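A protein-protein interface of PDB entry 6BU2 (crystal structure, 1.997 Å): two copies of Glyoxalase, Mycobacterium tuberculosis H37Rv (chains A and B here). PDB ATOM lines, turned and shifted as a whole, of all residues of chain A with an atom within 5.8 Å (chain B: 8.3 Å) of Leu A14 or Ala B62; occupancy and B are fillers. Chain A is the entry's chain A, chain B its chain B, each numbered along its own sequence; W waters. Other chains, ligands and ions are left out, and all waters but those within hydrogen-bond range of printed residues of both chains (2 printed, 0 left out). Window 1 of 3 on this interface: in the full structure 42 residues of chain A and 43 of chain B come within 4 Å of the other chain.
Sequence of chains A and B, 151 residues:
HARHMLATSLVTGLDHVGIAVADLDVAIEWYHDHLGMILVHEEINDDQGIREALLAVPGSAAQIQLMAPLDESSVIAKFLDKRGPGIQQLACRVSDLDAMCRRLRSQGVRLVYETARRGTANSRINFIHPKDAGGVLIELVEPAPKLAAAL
Leu A14 touches Ala B62, but with the chains exchanged Ala A62 does not touch Leu B14 (4.7 Å). Val A17 touches its own counterpart, Val B17. Positions printed for both chains: 13, 14, 15, 16, 17, 61, 62, 63, 90, 91 and 93.
Of the 23 printed residues of chain B, 10 touch a printed residue of chain A. Printed residues of chain B that touch a printed residue of chain A: Arg B3, Val B17, Leu B35, Met B37, Val B57, Pro B58, Gly B59, Ser B60, Ala B62 and Ile B64. Hydrophobic or aromatic side chains of chain B within 4 Å of the printed part of chain A: Val B17, Met B37, Val B57, Ala B62 and Ile B64. Hydrophobic or aromatic side chains of chain A that line the printed part of chain B: Val A11, Leu A14, Val A17 and Leu A90. Among the printed residues, 13 pairs touch across the chains. Among the printed residues, no Asp or Glu carboxylate lies within 4 Å of a Lys or Arg side-chain nitrogen of the other chain.
Among the printed residues, merely in contact across the chains: Ala A61 with Arg B3 (3.5 Å), Val A11 with Leu B35 (3.6 Å), Gly A13 with Ser B60 (3.6 Å), Val A17 with Val B17 (3.7 Å), Leu A14 with Ala B62 (3.7 Å), Val A11 with Val B57 (3.7 Å), Leu A90 with Ile B64 (3.8 Å), Leu A14 with Ser B60 (3.8 Å), Cys A92 with Met B37 (3.9 Å), Val A11 with Pro B58 (3.9 Å), Gly A13 with Val B57 (3.9 Å) and Thr A12 with Pro B58 (3.98 Å).
Water W2 lies within hydrogen-bond range of the backbone carbonyl oxygen (O) of Pro B58 and the backbone carbonyl oxygen (O) of Val A11. Water W1 lies within hydrogen-bond range of the backbone carbonyl oxygen of Leu A14, the side-chain hydroxyl of Ser B60 and the guanidinium group of Arg A93.
The backbone carbonyl oxygen (O) of Gly B59 lies close to the backbone carbonyl oxygen (O) of Thr A12 (3.3 Å).
Gly A13 touches just these residues of chain B: Val B57 and Ser B60. Of chain B, only Ser B60 (3.8 Å) and Ala B62 (3.7 Å) come within 4 Å of Leu A14. Arg A93 touches none of the printed residues of chain B. Gly B13 touches none of the printed residues of chain A. Printed residues of chain A within 4 Å of Gly B59: Thr A12 (3.3 Å). Of the printed residues of chain A, Ser B60 touches Gly A13 (3.6 Å) and Leu A14 (3.8 Å). Ala B62 touches just one residue of chain A: Leu A14 (3.7 Å). The nearest residue of chain A that does not touch Ala B62 is Ala A62 (5.4 Å). The nearest printed residue of chain B that does not touch Cys A92 is Leu B35 (4.4 Å).
The backbone NH (N) of Thr A12 is in hydrogen-bond range of the backbone carbonyl oxygen (O) of Arg A93, 2.8 Å away. The backbone carbonyl oxygen of Gln B63 is in hydrogen-bond range of the backbone NH of Val B17, at 3.0 Å. The backbone NH of Leu B55 sits at hydrogen-bond distance from the backbone carbonyl oxygen of Ile B64, 2.8 Å away. OG of Ser B60 is in hydrogen-bond range of N of Ala B62, at 3.3 Å. O of Val B17 is in hydrogen-bond range of N of Gln B65 (2.9 Å). The backbone NH (N) of Val A17 is in hydrogen-bond range of the backbone carbonyl oxygen (O) of Gln A63, at 2.9 Å.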
ATOM      1  N   VAL A  11      17.890  19.473 -20.351  1.00  0.00           N
ATOM      2  CA  VAL A  11      17.764  19.547 -18.898  1.00  0.00           C
ATOM      3  C   VAL A  11      16.741  18.513 -18.442  1.00  0.00           C
ATOM      4  O   VAL A  11      15.660  18.381 -19.033  1.00  0.00           O
ATOM      5  CB  VAL A  11      17.370  20.968 -18.471  1.00  0.00           C
ATOM      6  CG1 VAL A  11      17.041  21.024 -16.967  1.00  0.00           C
ATOM      7  CG2 VAL A  11      18.488  21.948 -18.829  1.00  0.00           C
ATOM      8  N   THR A  12      17.089  17.758 -17.406  1.00  0.00           N
ATOM      9  CA  THR A  12      16.218  16.721 -16.878  1.00  0.00           C
ATOM     10  C   THR A  12      15.801  16.998 -15.447  1.00  0.00           C
ATOM     11  O   THR A  12      15.107  16.166 -14.849  1.00  0.00           O
ATOM     12  CB  THR A  12      16.903  15.347 -16.954  1.00  0.00           C
ATOM     13  OG1 THR A  12      18.084  15.353 -16.141  1.00  0.00           O
ATOM     14  CG2 THR A  12      17.270  15.006 -18.404  1.00  0.00           C
ATOM     15  N   GLY A  13      16.219  18.120 -14.884  1.00  0.00           N
ATOM     16  CA  GLY A  13      15.844  18.490 -13.532  1.00  0.00           C
ATOM     17  C   GLY A  13      16.896  19.392 -12.921  1.00  0.00           C
ATOM     18  O   GLY A  13      17.851  19.801 -13.571  1.00  0.00           O
ATOM     19  N   LEU A  14      16.692  19.704 -11.640  1.00  0.00           N
ATOM     20  CA  LEU A  14      17.660  20.489 -10.880  1.00  0.00           C
ATOM     21  C   LEU A  14      18.593  19.538 -10.147  1.00  0.00           C
ATOM     22  O   LEU A  14      18.143  18.698  -9.356  1.00  0.00           O
ATOM     23  CB  LEU A  14      16.972  21.433  -9.896  1.00  0.00           C
ATOM     24  CG  LEU A  14      16.179  22.602 -10.489  1.00  0.00           C
ATOM     25  CD1 LEU A  14      15.656  23.513  -9.376  1.00  0.00           C
ATOM     26  CD2 LEU A  14      17.003  23.407 -11.495  1.00  0.00           C
ATOM     27  N   ASP A  15      19.893  19.660 -10.416  1.00  0.00           N
ATOM     28  CA  ASP A  15      20.842  18.788  -9.744  1.00  0.00           C
ATOM     29  C   ASP A  15      21.078  19.222  -8.303  1.00  0.00           C
ATOM     30  O   ASP A  15      21.067  18.388  -7.391  1.00  0.00           O
ATOM     31  CB  ASP A  15      22.169  18.747 -10.486  1.00  0.00           C
ATOM     32  CG  ASP A  15      23.080  17.719  -9.908  1.00  0.00           C
ATOM     33  OD1 ASP A  15      23.885  18.068  -9.009  1.00  0.00           O
ATOM     34  OD2 ASP A  15      22.940  16.546 -10.306  1.00  0.00           O
ATOM     35  N   HIS A  16      21.326  20.510  -8.082  1.00  0.00           N
ATOM     36  CA  HIS A  16      21.585  20.973  -6.726  1.00  0.00           C
ATOM     37  C   HIS A  16      21.547  22.493  -6.692  1.00  0.00           C
ATOM     38  O   HIS A  16      21.611  23.174  -7.723  1.00  0.00           O
ATOM     39  CB  HIS A  16      22.927  20.453  -6.171  1.00  0.00           C
ATOM     40  CG  HIS A  16      24.130  20.945  -6.915  1.00  0.00           C
ATOM     41  ND1 HIS A  16      24.795  20.178  -7.848  1.00  0.00           N
ATOM     42  CD2 HIS A  16      24.790  22.127  -6.860  1.00  0.00           C
ATOM     43  CE1 HIS A  16      25.816  20.863  -8.333  1.00  0.00           C
ATOM     44  NE2 HIS A  16      25.834  22.051  -7.753  1.00  0.00           N
ATOM     45  N   VAL A  17      21.456  23.021  -5.474  1.00  0.00           N
ATOM     46  CA  VAL A  17      21.653  24.439  -5.214  1.00  0.00           C
ATOM     47  C   VAL A  17      22.926  24.572  -4.390  1.00  0.00           C
ATOM     48  O   VAL A  17      23.051  23.939  -3.331  1.00  0.00           O
ATOM     49  CB  VAL A  17      20.445  25.055  -4.490  1.00  0.00           C
ATOM     50  CG1 VAL A  17      20.602  26.559  -4.373  1.00  0.00           C
ATOM     51  CG2 VAL A  17      19.155  24.732  -5.229  1.00  0.00           C
ATOM     52  N   ALA A  61      14.611  15.025  -5.453  1.00  0.00           N
ATOM     53  CA  ALA A  61      15.835  14.589  -6.122  1.00  0.00           C
ATOM     54  C   ALA A  61      16.931  15.652  -6.111  1.00  0.00           C
ATOM     55  O   ALA A  61      18.110  15.312  -6.267  1.00  0.00           O
ATOM     56  CB  ALA A  61      15.517  14.181  -7.567  1.00  0.00           C
ATOM     57  N   ALA A  62      16.584  16.921  -5.936  1.00  0.00           N
ATOM     58  CA  ALA A  62      17.589  17.977  -5.909  1.00  0.00           C
ATOM     59  C   ALA A  62      18.267  18.037  -4.541  1.00  0.00           C
ATOM     60  O   ALA A  62      17.654  17.749  -3.516  1.00  0.00           O
ATOM     61  CB  ALA A  62      16.958  19.325  -6.257  1.00  0.00           C
ATOM     62  N   GLN A  63      19.565  18.349  -4.544  1.00  0.00           N
ATOM     63  CA  GLN A  63      20.381  18.400  -3.343  1.00  0.00           C
ATOM     64  C   GLN A  63      20.784  19.832  -3.014  1.00  0.00           C
ATOM     65  O   GLN A  63      20.684  20.744  -3.839  1.00  0.00           O
ATOM     66  CB  GLN A  63      21.640  17.530  -3.500  1.00  0.00           C
ATOM     67  CG  GLN A  63      21.356  16.050  -3.749  1.00  0.00           C
ATOM     68  CD  GLN A  63      22.630  15.212  -3.826  1.00  0.00           C
ATOM     69  OE1 GLN A  63      23.693  15.704  -4.215  1.00  0.00           O
ATOM     70  NE2 GLN A  63      22.525  13.942  -3.449  1.00  0.00           N
ATOM     71  N   LEU A  90      23.138  27.687  -9.175  1.00  0.00           N
ATOM     72  CA  LEU A  90      22.019  26.824  -9.525  1.00  0.00           C
ATOM     73  C   LEU A  90      22.524  25.799 -10.535  1.00  0.00           C
ATOM     74  O   LEU A  90      23.046  26.183 -11.589  1.00  0.00           O
ATOM     75  CB  LEU A  90      20.915  27.672 -10.154  1.00  0.00           C
ATOM     76  CG  LEU A  90      19.776  26.935 -10.814  1.00  0.00           C
ATOM     77  CD1 LEU A  90      18.894  26.412  -9.720  1.00  0.00           C
ATOM     78  CD2 LEU A  90      19.027  27.875 -11.725  1.00  0.00           C
ATOM     79  N   ALA A  91      22.369  24.512 -10.235  1.00  0.00           N
ATOM     80  CA  ALA A  91      22.894  23.454 -11.100  1.00  0.00           C
ATOM     81  C   ALA A  91      21.742  22.677 -11.718  1.00  0.00           C
ATOM     82  O   ALA A  91      20.927  22.091 -10.996  1.00  0.00           O
ATOM     83  CB  ALA A  91      23.814  22.519 -10.318  1.00  0.00           C
ATOM     84  N   CYS A  92      21.673  22.686 -13.046  1.00  0.00           N
ATOM     85  CA  CYS A  92      20.718  21.885 -13.796  1.00  0.00           C
ATOM     86  C   CYS A  92      21.331  20.531 -14.119  1.00  0.00           C
ATOM     87  O   CYS A  92      22.486  20.455 -14.560  1.00  0.00           O
ATOM     88  CB  CYS A  92      20.323  22.593 -15.099  1.00  0.00           C
ATOM     89  SG  CYS A  92      19.460  24.184 -14.859  1.00  0.00           S
ATOM     90  N   ARG A  93      20.555  19.465 -13.917  1.00  0.00           N
ATOM     91  CA  ARG A  93      20.965  18.149 -14.385  1.00  0.00           C
ATOM     92  C   ARG A  93      20.653  18.025 -15.864  1.00  0.00           C
ATOM     93  O   ARG A  93      19.613  18.489 -16.339  1.00  0.00           O
ATOM     94  CB  ARG A  93      20.265  17.039 -13.602  1.00  0.00           C
ATOM     95  CG  ARG A  93      20.800  15.637 -13.912  1.00  0.00           C
ATOM     96  CD  ARG A  93      20.576  14.664 -12.756  1.00  0.00           C
ATOM     97  NE  ARG A  93      19.441  15.047 -11.920  1.00  0.00           N
ATOM     98  CZ  ARG A  93      18.163  14.792 -12.206  1.00  0.00           C
ATOM     99  NH1 ARG A  93      17.835  14.145 -13.321  1.00  0.00           N
ATOM    100  NH2 ARG A  93      17.206  15.193 -11.375  1.00  0.00           N
ATOM    101  N   ARG B   3      14.228  10.795  -3.303  1.00  0.00           N
ATOM    102  CA  ARG B   3      12.787  10.929  -3.486  1.00  0.00           C
ATOM    103  C   ARG B   3      12.018   9.848  -2.732  1.00  0.00           C
ATOM    104  O   ARG B   3      10.830  10.030  -2.441  1.00  0.00           O
ATOM    105  CB  ARG B   3      12.423  10.887  -4.975  1.00  0.00           C
ATOM    106  CG  ARG B   3      12.516  12.240  -5.683  1.00  0.00           C
ATOM    107  CD  ARG B   3      11.699  12.265  -6.977  1.00  0.00           C
ATOM    108  NE  ARG B   3      10.269  12.035  -6.737  1.00  0.00           N
ATOM    109  CZ  ARG B   3       9.348  12.993  -6.616  1.00  0.00           C
ATOM    110  NH1 ARG B   3       9.685  14.273  -6.715  1.00  0.00           N
ATOM    111  NH2 ARG B   3       8.080  12.665  -6.398  1.00  0.00           N
ATOM    112  N   GLY B  13      10.345  18.694   0.277  1.00  0.00           N
ATOM    113  CA  GLY B  13      11.087  18.968  -0.922  1.00  0.00           C
ATOM    114  C   GLY B  13      11.479  20.420  -1.145  1.00  0.00           C
ATOM    115  O   GLY B  13      11.314  21.245  -0.316  1.00  0.00           O
ATOM    116  N   LEU B  14      11.988  20.676  -2.323  1.00  0.00           N
ATOM    117  CA  LEU B  14      12.404  21.982  -2.738  1.00  0.00           C
ATOM    118  C   LEU B  14      11.281  22.600  -3.505  1.00  0.00           C
ATOM    119  O   LEU B  14      10.919  22.094  -4.517  1.00  0.00           O
ATOM    120  CB  LEU B  14      13.534  21.825  -3.700  1.00  0.00           C
ATOM    121  CG  LEU B  14      14.845  22.427  -3.360  1.00  0.00           C
ATOM    122  CD1 LEU B  14      14.616  23.911  -3.296  1.00  0.00           C
ATOM    123  CD2 LEU B  14      15.231  21.883  -2.014  1.00  0.00           C
ATOM    124  N   ASP B  15      10.753  23.699  -3.030  1.00  0.00           N
ATOM    125  CA  ASP B  15       9.646  24.354  -3.737  1.00  0.00           C
ATOM    126  C   ASP B  15      10.151  25.161  -4.924  1.00  0.00           C
ATOM    127  O   ASP B  15       9.632  25.024  -6.042  1.00  0.00           O
ATOM    128  CB  ASP B  15       8.843  25.278  -2.810  1.00  0.00           C
ATOM    129  CG  ASP B  15       7.595  25.832  -3.491  1.00  0.00           C
ATOM    130  OD1 ASP B  15       6.592  25.098  -3.492  1.00  0.00           O
ATOM    131  OD2 ASP B  15       7.591  26.989  -3.990  1.00  0.00           O
ATOM    132  N   HIS B  16      11.116  26.046  -4.691  1.00  0.00           N
ATOM    133  CA  HIS B  16      11.680  26.817  -5.790  1.00  0.00           C
ATOM    134  C   HIS B  16      13.017  27.410  -5.381  1.00  0.00           C
ATOM    135  O   HIS B  16      13.385  27.436  -4.203  1.00  0.00           O
ATOM    136  CB  HIS B  16      10.722  27.923  -6.269  1.00  0.00           C
ATOM    137  CG  HIS B  16      10.379  28.948  -5.229  1.00  0.00           C
ATOM    138  ND1 HIS B  16       9.218  28.890  -4.481  1.00  0.00           N
ATOM    139  CD2 HIS B  16      11.020  30.076  -4.838  1.00  0.00           C
ATOM    140  CE1 HIS B  16       9.162  29.938  -3.676  1.00  0.00           C
ATOM    141  NE2 HIS B  16      10.250  30.667  -3.864  1.00  0.00           N
ATOM    142  N   VAL B  17      13.730  27.907  -6.390  1.00  0.00           N
ATOM    143  CA  VAL B  17      14.888  28.774  -6.218  1.00  0.00           C
ATOM    144  C   VAL B  17      14.501  30.145  -6.754  1.00  0.00           C
ATOM    145  O   VAL B  17      14.077  30.278  -7.904  1.00  0.00           O
ATOM    146  CB  VAL B  17      16.120  28.204  -6.949  1.00  0.00           C
ATOM    147  CG1 VAL B  17      17.352  29.037  -6.660  1.00  0.00           C
ATOM    148  CG2 VAL B  17      16.363  26.756  -6.536  1.00  0.00           C
ATOM    149  N   LEU B  35      17.429  27.157 -21.411  1.00  0.00           N
ATOM    150  CA  LEU B  35      17.357  26.034 -20.484  1.00  0.00           C
ATOM    151  C   LEU B  35      16.101  25.192 -20.632  1.00  0.00           C
ATOM    152  O   LEU B  35      15.944  24.217 -19.892  1.00  0.00           O
ATOM    153  CB  LEU B  35      17.475  26.513 -19.027  1.00  0.00           C
ATOM    154  CG  LEU B  35      18.793  27.237 -18.712  1.00  0.00           C
ATOM    155  CD1 LEU B  35      18.791  27.834 -17.310  1.00  0.00           C
ATOM    156  CD2 LEU B  35      19.981  26.295 -18.911  1.00  0.00           C
ATOM    157  N   MET B  37      13.105  25.880 -19.710  1.00  0.00           N
ATOM    158  CA  MET B  37      12.162  26.086 -18.627  1.00  0.00           C
ATOM    159  C   MET B  37      10.892  26.676 -19.191  1.00  0.00           C
ATOM    160  O   MET B  37      10.932  27.398 -20.115  1.00  0.00           O
ATOM    161  CB  MET B  37      12.775  26.922 -17.511  1.00  0.00           C
ATOM    162  CG  MET B  37      14.122  26.405 -17.059  1.00  0.00           C
ATOM    163  SD  MET B  37      14.684  27.083 -15.516  1.00  0.00           S
ATOM    164  CE  MET B  37      16.180  26.200 -15.285  1.00  0.00           C
ATOM    165  N   LEU B  54       6.900  32.041 -12.466  1.00  0.00           N
ATOM    166  CA  LEU B  54       7.252  30.701 -12.019  1.00  0.00           C
ATOM    167  C   LEU B  54       7.553  29.850 -13.240  1.00  0.00           C
ATOM    168  O   LEU B  54       6.702  29.712 -14.124  1.00  0.00           O
ATOM    169  CB  LEU B  54       6.117  30.082 -11.201  1.00  0.00           C
ATOM    170  CG  LEU B  54       6.162  30.403  -9.706  1.00  0.00           C
ATOM    171  CD1 LEU B  54       4.863  29.986  -9.042  1.00  0.00           C
ATOM    172  CD2 LEU B  54       7.368  29.712  -9.041  1.00  0.00           C
ATOM    173  N   LEU B  55       8.748  29.267 -13.278  1.00  0.00           N
ATOM    174  CA  LEU B  55       9.190  28.460 -14.408  1.00  0.00           C
ATOM    175  C   LEU B  55       9.279  27.013 -13.967  1.00  0.00           C
ATOM    176  O   LEU B  55       9.965  26.698 -12.990  1.00  0.00           O
ATOM    177  CB  LEU B  55      10.547  28.922 -14.940  1.00  0.00           C
ATOM    178  CG  LEU B  55      10.705  30.418 -15.211  1.00  0.00           C
ATOM    179  CD1 LEU B  55      12.066  30.695 -15.863  1.00  0.00           C
ATOM    180  CD2 LEU B  55       9.559  30.938 -16.086  1.00  0.00           C
ATOM    181  N   ALA B  56       8.593  26.144 -14.684  1.00  0.00           N
ATOM    182  CA  ALA B  56       8.739  24.725 -14.445  1.00  0.00           C
ATOM    183  C   ALA B  56      10.015  24.238 -15.112  1.00  0.00           C
ATOM    184  O   ALA B  56      10.495  24.820 -16.091  1.00  0.00           O
ATOM    185  CB  ALA B  56       7.522  23.959 -14.974  1.00  0.00           C
ATOM    186  N   VAL B  57      10.595  23.200 -14.535  1.00  0.00           N
ATOM    187  CA  VAL B  57      11.739  22.496 -15.086  1.00  0.00           C
ATOM    188  C   VAL B  57      11.263  21.107 -15.449  1.00  0.00           C
ATOM    189  O   VAL B  57      11.138  20.242 -14.567  1.00  0.00           O
ATOM    190  CB  VAL B  57      12.910  22.447 -14.090  1.00  0.00           C
ATOM    191  CG1 VAL B  57      14.167  21.846 -14.725  1.00  0.00           C
ATOM    192  CG2 VAL B  57      13.200  23.828 -13.504  1.00  0.00           C
ATOM    193  N   PRO B  58      10.900  20.863 -16.707  1.00  0.00           N
ATOM    194  CA  PRO B  58      10.276  19.587 -17.066  1.00  0.00           C
ATOM    195  C   PRO B  58      11.185  18.427 -16.683  1.00  0.00           C
ATOM    196  O   PRO B  58      12.401  18.476 -16.890  1.00  0.00           O
ATOM    197  CB  PRO B  58      10.073  19.697 -18.582  1.00  0.00           C
ATOM    198  CG  PRO B  58       9.970  21.167 -18.833  1.00  0.00           C
ATOM    199  CD  PRO B  58      10.953  21.790 -17.857  1.00  0.00           C
ATOM    200  N   GLY B  59      10.584  17.405 -16.070  1.00  0.00           N
ATOM    201  CA  GLY B  59      11.319  16.346 -15.409  1.00  0.00           C
ATOM    202  C   GLY B  59      11.599  16.581 -13.940  1.00  0.00           C
ATOM    203  O   GLY B  59      12.219  15.727 -13.299  1.00  0.00           O
ATOM    204  N   SER B  60      11.162  17.707 -13.386  1.00  0.00           N
ATOM    205  CA  SER B  60      11.487  18.068 -12.016  1.00  0.00           C
ATOM    206  C   SER B  60      10.256  18.666 -11.337  1.00  0.00           C
ATOM    207  O   SER B  60       9.338  19.166 -11.988  1.00  0.00           O
ATOM    208  CB  SER B  60      12.668  19.057 -11.976  1.00  0.00           C
ATOM    209  OG  SER B  60      12.996  19.436 -10.647  1.00  0.00           O
ATOM    210  N   ALA B  61      10.250  18.607 -10.008  1.00  0.00           N
ATOM    211  CA  ALA B  61       9.199  19.239  -9.224  1.00  0.00           C
ATOM    212  C   ALA B  61       9.573  20.638  -8.755  1.00  0.00           C
ATOM    213  O   ALA B  61       8.682  21.436  -8.455  1.00  0.00           O
ATOM    214  CB  ALA B  61       8.839  18.372  -8.009  1.00  0.00           C
ATOM    215  N   ALA B  62      10.857  20.963  -8.687  1.00  0.00           N
ATOM    216  CA  ALA B  62      11.239  22.280  -8.209  1.00  0.00           C
ATOM    217  C   ALA B  62      11.129  23.302  -9.336  1.00  0.00           C
ATOM    218  O   ALA B  62      11.212  22.974 -10.527  1.00  0.00           O
ATOM    219  CB  ALA B  62      12.653  22.267  -7.627  1.00  0.00           C
ATOM    220  N   GLN B  63      10.888  24.548  -8.955  1.00  0.00           N
ATOM    221  CA  GLN B  63      10.699  25.593  -9.937  1.00  0.00           C
ATOM    222  C   GLN B  63      11.793  26.632  -9.809  1.00  0.00           C
ATOM    223  O   GLN B  63      12.522  26.686  -8.814  1.00  0.00           O
ATOM    224  CB  GLN B  63       9.323  26.246  -9.796  1.00  0.00           C
ATOM    225  CG  GLN B  63       8.171  25.263  -9.991  1.00  0.00           C
ATOM    226  CD  GLN B  63       6.815  25.940  -9.876  1.00  0.00           C
ATOM    227  OE1 GLN B  63       6.546  26.650  -8.907  1.00  0.00           O
ATOM    228  NE2 GLN B  63       5.956  25.721 -10.864  1.00  0.00           N
ATOM    229  N   ILE B  64      11.926  27.431 -10.860  1.00  0.00           N
ATOM    230  CA  ILE B  64      12.676  28.676 -10.813  1.00  0.00           C
ATOM    231  C   ILE B  64      11.672  29.814 -10.673  1.00  0.00           C
ATOM    232  O   ILE B  64      10.718  29.906 -11.456  1.00  0.00           O
ATOM    233  CB  ILE B  64      13.539  28.850 -12.073  1.00  0.00           C
ATOM    234  CG1 ILE B  64      14.585  27.735 -12.151  1.00  0.00           C
ATOM    235  CG2 ILE B  64      14.175  30.237 -12.096  1.00  0.00           C
ATOM    236  CD1 ILE B  64      15.362  27.573 -10.919  1.00  0.00           C
ATOM    237  N   GLN B  65      11.868  30.668  -9.681  1.00  0.00           N
ATOM    238  CA  GLN B  65      10.997  31.825  -9.453  1.00  0.00           C
ATOM    239  C   GLN B  65      11.790  33.087  -9.772  1.00  0.00           C
ATOM    240  O   GLN B  65      12.584  33.557  -8.954  1.00  0.00           O
ATOM    241  CB  GLN B  65      10.478  31.851  -8.020  1.00  0.00           C
ATOM    242  CG  GLN B  65       9.614  33.059  -7.648  1.00  0.00           C
ATOM    243  CD  GLN B  65       8.803  32.783  -6.365  1.00  0.00           C
ATOM    244  OE1 GLN B  65       8.016  31.843  -6.321  1.00  0.00           O
ATOM    245  NE2 GLN B  65       9.012  33.579  -5.334  1.00  0.00           N
ATOM    246  N   LEU B  90      16.215  30.387  -1.292  1.00  0.00           N
ATOM    247  CA  LEU B  90      15.976  28.953  -1.393  1.00  0.00           C
ATOM    248  C   LEU B  90      14.661  28.648  -0.677  1.00  0.00           C
ATOM    249  O   LEU B  90      14.498  29.010   0.495  1.00  0.00           O
ATOM    250  CB  LEU B  90      17.126  28.195  -0.723  1.00  0.00           C
ATOM    251  CG  LEU B  90      16.934  26.693  -0.543  1.00  0.00           C
ATOM    252  CD1 LEU B  90      17.096  26.015  -1.867  1.00  0.00           C
ATOM    253  CD2 LEU B  90      17.928  26.133   0.446  1.00  0.00           C
ATOM    254  N   ALA B  91      13.719  27.995  -1.356  1.00  0.00           N
ATOM    255  CA  ALA B  91      12.395  27.778  -0.766  1.00  0.00           C
ATOM    256  C   ALA B  91      12.138  26.285  -0.585  1.00  0.00           C
ATOM    257  O   ALA B  91      12.045  25.541  -1.570  1.00  0.00           O
ATOM    258  CB  ALA B  91      11.305  28.416  -1.623  1.00  0.00           C
ATOM    259  N   ARG B  93       9.636  23.276   0.341  1.00  0.00           N
ATOM    260  CA  ARG B  93       8.228  22.927   0.452  1.00  0.00           C
ATOM    261  C   ARG B  93       8.005  22.188   1.765  1.00  0.00           C
ATOM    262  O   ARG B  93       8.824  21.353   2.169  1.00  0.00           O
ATOM    263  CB  ARG B  93       7.775  22.061  -0.728  1.00  0.00           C
ATOM    264  CG  ARG B  93       6.233  21.991  -0.884  1.00  0.00           C
ATOM    265  CD  ARG B  93       5.787  20.995  -1.962  1.00  0.00           C
ATOM    266  NE  ARG B  93       6.427  21.264  -3.245  1.00  0.00           N
ATOM    267  CZ  ARG B  93       5.959  22.111  -4.156  1.00  0.00           C
ATOM    268  NH1 ARG B  93       6.622  22.299  -5.290  1.00  0.00           N
ATOM    269  NH2 ARG B  93       4.830  22.770  -3.936  1.00  0.00           N
HETATM  270  O   HOH W   1      15.326  17.486  -9.735  1.00  0.00           O
HETATM  271  O   HOH W   2      13.585  20.193 -18.621  1.00  0.00           O
